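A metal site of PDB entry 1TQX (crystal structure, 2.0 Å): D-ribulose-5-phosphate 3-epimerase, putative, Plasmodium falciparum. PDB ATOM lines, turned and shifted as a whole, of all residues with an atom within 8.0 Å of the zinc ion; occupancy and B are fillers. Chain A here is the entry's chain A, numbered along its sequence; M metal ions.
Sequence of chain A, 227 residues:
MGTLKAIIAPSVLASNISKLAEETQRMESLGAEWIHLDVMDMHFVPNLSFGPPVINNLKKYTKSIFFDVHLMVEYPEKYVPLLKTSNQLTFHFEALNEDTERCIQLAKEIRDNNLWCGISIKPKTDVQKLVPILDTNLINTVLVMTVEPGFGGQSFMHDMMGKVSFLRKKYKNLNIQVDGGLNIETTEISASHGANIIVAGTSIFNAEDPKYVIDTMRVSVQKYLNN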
ATOM      1  N   ALA A   9       3.693 -18.904  -0.923  1.00  0.00           N
ATOM      2  CA  ALA A   9       4.207 -19.963  -1.787  1.00  0.00           C
ATOM      3  C   ALA A   9       3.104 -20.941  -2.210  1.00  0.00           C
ATOM      4  O   ALA A   9       2.845 -21.924  -1.519  1.00  0.00           O
ATOM      5  CB  ALA A   9       5.322 -20.709  -1.068  1.00  0.00           C
ATOM      6  N   SER A  11       1.119 -23.952  -3.623  1.00  0.00           N
ATOM      7  CA  SER A  11       1.498 -25.355  -3.779  1.00  0.00           C
ATOM      8  C   SER A  11       0.919 -25.912  -5.069  1.00  0.00           C
ATOM      9  O   SER A  11      -0.284 -26.104  -5.186  1.00  0.00           O
ATOM     10  CB  SER A  11       0.985 -26.163  -2.581  1.00  0.00           C
ATOM     11  OG  SER A  11       1.421 -27.511  -2.658  1.00  0.00           O
ATOM     12  N   LEU A  13       0.718 -28.753  -6.249  1.00  0.00           N
ATOM     13  CA  LEU A  13       0.055 -30.055  -6.136  1.00  0.00           C
ATOM     14  C   LEU A  13      -1.453 -29.860  -6.376  1.00  0.00           C
ATOM     15  O   LEU A  13      -2.120 -30.753  -6.896  1.00  0.00           O
ATOM     16  CB  LEU A  13       0.277 -30.623  -4.726  1.00  0.00           C
ATOM     17  CG  LEU A  13      -0.174 -32.048  -4.421  1.00  0.00           C
ATOM     18  CD1 LEU A  13       0.813 -33.049  -5.016  1.00  0.00           C
ATOM     19  CD2 LEU A  13      -0.250 -32.241  -2.911  1.00  0.00           C
ATOM     20  N   HIS A  36       5.848 -23.602  -4.390  1.00  0.00           N
ATOM     21  CA  HIS A  36       6.051 -24.762  -3.516  1.00  0.00           C
ATOM     22  C   HIS A  36       5.851 -26.067  -4.270  1.00  0.00           C
ATOM     23  O   HIS A  36       4.751 -26.370  -4.733  1.00  0.00           O
ATOM     24  CB  HIS A  36       5.079 -24.682  -2.334  1.00  0.00           C
ATOM     25  CG  HIS A  36       5.414 -25.598  -1.213  1.00  0.00           C
ATOM     26  ND1 HIS A  36       6.463 -25.356  -0.346  1.00  0.00           N
ATOM     27  CD2 HIS A  36       4.847 -26.765  -0.801  1.00  0.00           C
ATOM     28  CE1 HIS A  36       6.530 -26.326   0.541  1.00  0.00           C
ATOM     29  NE2 HIS A  36       5.564 -27.199   0.293  1.00  0.00           N
ATOM     30  N   LEU A  37       6.925 -26.849  -4.350  1.00  0.00           N
ATOM     31  CA  LEU A  37       6.912 -28.109  -5.086  1.00  0.00           C
ATOM     32  C   LEU A  37       6.964 -29.351  -4.187  1.00  0.00           C
ATOM     33  O   LEU A  37       8.015 -29.686  -3.641  1.00  0.00           O
ATOM     34  CB  LEU A  37       8.107 -28.120  -6.056  1.00  0.00           C
ATOM     35  CG  LEU A  37       8.170 -26.873  -6.955  1.00  0.00           C
ATOM     36  CD1 LEU A  37       9.586 -26.655  -7.506  1.00  0.00           C
ATOM     37  CD2 LEU A  37       7.158 -27.022  -8.079  1.00  0.00           C
ATOM     38  N   ASP A  38       5.833 -30.027  -4.059  1.00  0.00           N
ATOM     39  CA  ASP A  38       5.742 -31.226  -3.221  1.00  0.00           C
ATOM     40  C   ASP A  38       6.165 -32.514  -3.937  1.00  0.00           C
ATOM     41  O   ASP A  38       5.517 -32.941  -4.885  1.00  0.00           O
ATOM     42  CB  ASP A  38       4.315 -31.412  -2.696  1.00  0.00           C
ATOM     43  CG  ASP A  38       3.940 -30.386  -1.653  1.00  0.00           C
ATOM     44  OD1 ASP A  38       4.750 -30.136  -0.750  1.00  0.00           O
ATOM     45  OD2 ASP A  38       2.822 -29.840  -1.717  1.00  0.00           O
ATOM     46  N   VAL A  39       7.247 -33.125  -3.450  1.00  0.00           N
ATOM     47  CA  VAL A  39       7.763 -34.367  -4.013  1.00  0.00           C
ATOM     48  C   VAL A  39       7.398 -35.501  -3.058  1.00  0.00           C
ATOM     49  O   VAL A  39       7.799 -35.499  -1.891  1.00  0.00           O
ATOM     50  CB  VAL A  39       9.302 -34.298  -4.158  1.00  0.00           C
ATOM     51  CG1 VAL A  39       9.838 -35.572  -4.794  1.00  0.00           C
ATOM     52  CG2 VAL A  39       9.679 -33.080  -5.021  1.00  0.00           C
ATOM     53  N   MET A  40       6.631 -36.481  -3.551  1.00  0.00           N
ATOM     54  CA  MET A  40       6.176 -37.620  -2.758  1.00  0.00           C
ATOM     55  C   MET A  40       6.564 -38.915  -3.486  1.00  0.00           C
ATOM     56  O   MET A  40       6.400 -39.006  -4.695  1.00  0.00           O
ATOM     57  CB  MET A  40       4.657 -37.537  -2.572  1.00  0.00           C
ATOM     58  CG  MET A  40       4.200 -36.202  -1.991  1.00  0.00           C
ATOM     59  SD  MET A  40       2.414 -36.048  -2.062  1.00  0.00           S
ATOM     60  CE  MET A  40       2.163 -34.522  -1.146  1.00  0.00           C
ATOM     61  N   ASP A  68      10.927 -23.760  -4.125  1.00  0.00           N
ATOM     62  CA  ASP A  68      10.866 -24.316  -2.779  1.00  0.00           C
ATOM     63  C   ASP A  68      10.387 -25.770  -2.855  1.00  0.00           C
ATOM     64  O   ASP A  68       9.200 -26.049  -3.034  1.00  0.00           O
ATOM     65  CB  ASP A  68       9.937 -23.437  -1.946  1.00  0.00           C
ATOM     66  CG  ASP A  68       9.693 -23.967  -0.559  1.00  0.00           C
ATOM     67  OD1 ASP A  68      10.637 -24.476   0.077  1.00  0.00           O
ATOM     68  OD2 ASP A  68       8.541 -23.845  -0.103  1.00  0.00           O
ATOM     69  N   VAL A  69      11.334 -26.705  -2.718  1.00  0.00           N
ATOM     70  CA  VAL A  69      11.038 -28.131  -2.823  1.00  0.00           C
ATOM     71  C   VAL A  69      10.854 -28.821  -1.480  1.00  0.00           C
ATOM     72  O   VAL A  69      11.763 -28.857  -0.650  1.00  0.00           O
ATOM     73  CB  VAL A  69      12.152 -28.873  -3.611  1.00  0.00           C
ATOM     74  CG1 VAL A  69      11.712 -30.301  -3.894  1.00  0.00           C
ATOM     75  CG2 VAL A  69      12.444 -28.126  -4.919  1.00  0.00           C
ATOM     76  N   HIS A  70       9.664 -29.387  -1.269  1.00  0.00           N
ATOM     77  CA  HIS A  70       9.347 -30.098  -0.043  1.00  0.00           C
ATOM     78  C   HIS A  70       9.506 -31.591  -0.341  1.00  0.00           C
ATOM     79  O   HIS A  70       8.675 -32.179  -1.034  1.00  0.00           O
ATOM     80  CB  HIS A  70       7.905 -29.794   0.392  1.00  0.00           C
ATOM     81  CG  HIS A  70       7.500 -30.472   1.664  1.00  0.00           C
ATOM     82  ND1 HIS A  70       6.230 -30.352   2.194  1.00  0.00           N
ATOM     83  CD2 HIS A  70       8.177 -31.291   2.501  1.00  0.00           C
ATOM     84  CE1 HIS A  70       6.145 -31.066   3.302  1.00  0.00           C
ATOM     85  NE2 HIS A  70       7.310 -31.651   3.503  1.00  0.00           N
ATOM     86  N   LEU A  71      10.568 -32.191   0.193  1.00  0.00           N
ATOM     87  CA  LEU A  71      10.850 -33.599  -0.026  1.00  0.00           C
ATOM     88  C   LEU A  71      10.169 -34.531   0.964  1.00  0.00           C
ATOM     89  O   LEU A  71      10.695 -34.807   2.033  1.00  0.00           O
ATOM     90  CB  LEU A  71      12.370 -33.830   0.017  1.00  0.00           C
ATOM     91  CG  LEU A  71      13.186 -33.043  -1.016  1.00  0.00           C
ATOM     92  CD1 LEU A  71      14.663 -33.064  -0.654  1.00  0.00           C
ATOM     93  CD2 LEU A  71      12.951 -33.651  -2.399  1.00  0.00           C
ATOM     94  N   MET A  72       8.969 -34.990   0.615  1.00  0.00           N
ATOM     95  CA  MET A  72       8.247 -35.937   1.477  1.00  0.00           C
ATOM     96  C   MET A  72       8.634 -37.290   0.916  1.00  0.00           C
ATOM     97  O   MET A  72       7.813 -38.006   0.342  1.00  0.00           O
ATOM     98  CB  MET A  72       6.729 -35.722   1.362  1.00  0.00           C
ATOM     99  CG  MET A  72       6.251 -34.472   2.084  1.00  0.00           C
ATOM    100  SD  MET A  72       4.504 -34.094   1.819  1.00  0.00           S
ATOM    101  CE  MET A  72       4.619 -32.898   0.501  1.00  0.00           C
ATOM    102  N   THR A  90      13.717 -28.913   1.415  1.00  0.00           N
ATOM    103  CA  THR A  90      13.210 -29.182   2.760  1.00  0.00           C
ATOM    104  C   THR A  90      12.989 -30.671   2.930  1.00  0.00           C
ATOM    105  O   THR A  90      12.207 -31.281   2.192  1.00  0.00           O
ATOM    106  CB  THR A  90      11.867 -28.435   2.997  1.00  0.00           C
ATOM    107  OG1 THR A  90      12.090 -27.019   2.923  1.00  0.00           O
ATOM    108  CG2 THR A  90      11.272 -28.778   4.364  1.00  0.00           C
ATOM    109  N   HIS A  92      12.315 -34.137   5.685  1.00  0.00           N
ATOM    110  CA  HIS A  92      11.611 -34.448   6.918  1.00  0.00           C
ATOM    111  C   HIS A  92      12.494 -34.994   8.036  1.00  0.00           C
ATOM    112  O   HIS A  92      13.325 -35.872   7.814  1.00  0.00           O
ATOM    113  CB  HIS A  92      10.461 -35.425   6.648  1.00  0.00           C
ATOM    114  CG  HIS A  92       9.175 -34.741   6.310  1.00  0.00           C
ATOM    115  ND1 HIS A  92       8.271 -34.330   7.271  1.00  0.00           N
ATOM    116  CD2 HIS A  92       8.676 -34.297   5.121  1.00  0.00           C
ATOM    117  CE1 HIS A  92       7.293 -33.659   6.702  1.00  0.00           C
ATOM    118  NE2 HIS A  92       7.519 -33.617   5.397  1.00  0.00           N
ATOM    119  N   SER A 120      11.214 -30.286   7.984  1.00  0.00           N
ATOM    120  CA  SER A 120       9.808 -30.364   8.312  1.00  0.00           C
ATOM    121  C   SER A 120       9.478 -31.414   9.368  1.00  0.00           C
ATOM    122  O   SER A 120      10.177 -32.414   9.507  1.00  0.00           O
ATOM    123  CB  SER A 120       8.992 -30.642   7.037  1.00  0.00           C
ATOM    124  OG  SER A 120       7.602 -30.642   7.295  1.00  0.00           O
ATOM    125  N   LEU A 143       9.356 -26.155   8.382  1.00  0.00           N
ATOM    126  CA  LEU A 143       8.024 -26.309   7.808  1.00  0.00           C
ATOM    127  C   LEU A 143       7.144 -27.088   8.782  1.00  0.00           C
ATOM    128  O   LEU A 143       7.309 -28.297   8.933  1.00  0.00           O
ATOM    129  CB  LEU A 143       8.131 -27.050   6.460  1.00  0.00           C
ATOM    130  CG  LEU A 143       6.923 -27.107   5.510  1.00  0.00           C
ATOM    131  CD1 LEU A 143       7.368 -27.809   4.217  1.00  0.00           C
ATOM    132  CD2 LEU A 143       5.770 -27.849   6.131  1.00  0.00           C
ATOM    133  N   MET A 145       3.944 -28.785   9.498  1.00  0.00           N
ATOM    134  CA  MET A 145       2.788 -29.329   8.805  1.00  0.00           C
ATOM    135  C   MET A 145       1.552 -29.049   9.660  1.00  0.00           C
ATOM    136  O   MET A 145       1.558 -29.331  10.855  1.00  0.00           O
ATOM    137  CB  MET A 145       2.906 -30.846   8.619  1.00  0.00           C
ATOM    138  CG  MET A 145       3.948 -31.302   7.609  1.00  0.00           C
ATOM    139  SD  MET A 145       3.702 -30.635   5.942  1.00  0.00           S
ATOM    140  CE  MET A 145       2.082 -31.264   5.532  1.00  0.00           C
ATOM    141  N   PRO A 149       0.547 -34.916   6.167  1.00  0.00           N
ATOM    142  CA  PRO A 149       1.090 -34.880   4.805  1.00  0.00           C
ATOM    143  C   PRO A 149       0.726 -36.014   3.860  1.00  0.00           C
ATOM    144  O   PRO A 149       0.605 -37.172   4.267  1.00  0.00           O
ATOM    145  CB  PRO A 149       2.598 -34.764   5.037  1.00  0.00           C
ATOM    146  CG  PRO A 149       2.786 -35.543   6.295  1.00  0.00           C
ATOM    147  CD  PRO A 149       1.629 -35.080   7.155  1.00  0.00           C
ATOM    148  N   GLY A 150       0.576 -35.677   2.587  1.00  0.00           N
ATOM    149  CA  GLY A 150       0.248 -36.670   1.576  1.00  0.00           C
ATOM    150  C   GLY A 150      -0.798 -36.175   0.591  1.00  0.00           C
ATOM    151  O   GLY A 150      -0.727 -36.472  -0.595  1.00  0.00           O
ATOM    152  N   GLN A 177       7.380 -21.775   8.198  1.00  0.00           N
ATOM    153  CA  GLN A 177       6.452 -22.060   7.116  1.00  0.00           C
ATOM    154  C   GLN A 177       5.333 -22.989   7.593  1.00  0.00           C
ATOM    155  O   GLN A 177       5.569 -23.917   8.378  1.00  0.00           O
ATOM    156  CB  GLN A 177       7.261 -22.710   5.980  1.00  0.00           C
ATOM    157  CG  GLN A 177       6.505 -22.989   4.697  1.00  0.00           C
ATOM    158  CD  GLN A 177       7.427 -23.508   3.612  1.00  0.00           C
ATOM    159  OE1 GLN A 177       8.236 -24.409   3.852  1.00  0.00           O
ATOM    160  NE2 GLN A 177       7.309 -22.959   2.394  1.00  0.00           N
ATOM    161  N   VAL A 178       4.102 -22.723   7.159  1.00  0.00           N
ATOM    162  CA  VAL A 178       2.963 -23.556   7.533  1.00  0.00           C
ATOM    163  C   VAL A 178       2.423 -24.137   6.246  1.00  0.00           C
ATOM    164  O   VAL A 178       2.411 -23.488   5.205  1.00  0.00           O
ATOM    165  CB  VAL A 178       1.870 -22.745   8.280  1.00  0.00           C
ATOM    166  CG1 VAL A 178       2.369 -22.418   9.679  1.00  0.00           C
ATOM    167  CG2 VAL A 178       1.533 -21.475   7.523  1.00  0.00           C
ATOM    168  N   ASP A 179       1.955 -25.385   6.321  1.00  0.00           N
ATOM    169  CA  ASP A 179       1.523 -26.081   5.124  1.00  0.00           C
ATOM    170  C   ASP A 179       0.405 -27.078   5.421  1.00  0.00           C
ATOM    171  O   ASP A 179       0.597 -28.011   6.196  1.00  0.00           O
ATOM    172  CB  ASP A 179       2.778 -26.779   4.567  1.00  0.00           C
ATOM    173  CG  ASP A 179       2.533 -27.586   3.306  1.00  0.00           C
ATOM    174  OD1 ASP A 179       3.546 -28.137   2.819  1.00  0.00           O
ATOM    175  OD2 ASP A 179       1.384 -27.673   2.814  1.00  0.00           O
ATOM    176  N   GLY A 180      -0.759 -26.869   4.817  1.00  0.00           N
ATOM    177  CA  GLY A 180      -1.887 -27.756   5.043  1.00  0.00           C
ATOM    178  C   GLY A 180      -3.142 -27.023   5.491  1.00  0.00           C
ATOM    179  O   GLY A 180      -3.279 -26.646   6.656  1.00  0.00           O
ATOM    180  N   VAL A 199       2.202 -21.650   2.711  1.00  0.00           N
ATOM    181  CA  VAL A 199       2.007 -22.567   1.600  1.00  0.00           C
ATOM    182  C   VAL A 199       0.506 -22.799   1.470  1.00  0.00           C
ATOM    183  O   VAL A 199      -0.138 -23.250   2.418  1.00  0.00           O
ATOM    184  CB  VAL A 199       2.703 -23.919   1.851  1.00  0.00           C
ATOM    185  CG1 VAL A 199       2.325 -24.917   0.758  1.00  0.00           C
ATOM    186  CG2 VAL A 199       4.219 -23.730   1.889  1.00  0.00           C
HETATM  187 ZN    ZN M   1       4.665 -29.081   1.089  1.00  0.00          ZN
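Residues that only touch the zinc ion: Met 72 (3.9 Å).
Within 4 Å of the zinc ion: His 36, Asp 38, His 70, Met 72 and Asp 179.
Along chain A the residues within 4 Å of the zinc ion span positions 36 to 179.
The nearest printed residue that does not touch the zinc ion is Leu 143 (4.3 Å).
The zinc ion is bound by OD1 of Asp 38, NE2 of His 36, OD1 of Asp 179 and ND1 of His 70.
The zinc ion has four donor atoms within binding distance.
The side-chain carboxylate of Asp 68 is in hydrogen-bond range of a ring nitrogen (ND1) of His 36, 2.6 Å away.
N of His 70 lies within hydrogen-bond range of O of Leu 37 (2.9 Å).
N of Met 72 lies within hydrogen-bond range of O of Val 39.
A ring nitrogen (NE2) of His 70 sits at hydrogen-bond distance from a ring nitrogen (NE2) of His 92.
The backbone carbonyl oxygen (O) of His 70 is in hydrogen-bond range of the backbone NH (N) of Val 39.
OD2 of Asp 38 lies within hydrogen-bond range of OG of Ser 11, at 2.9 Å.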
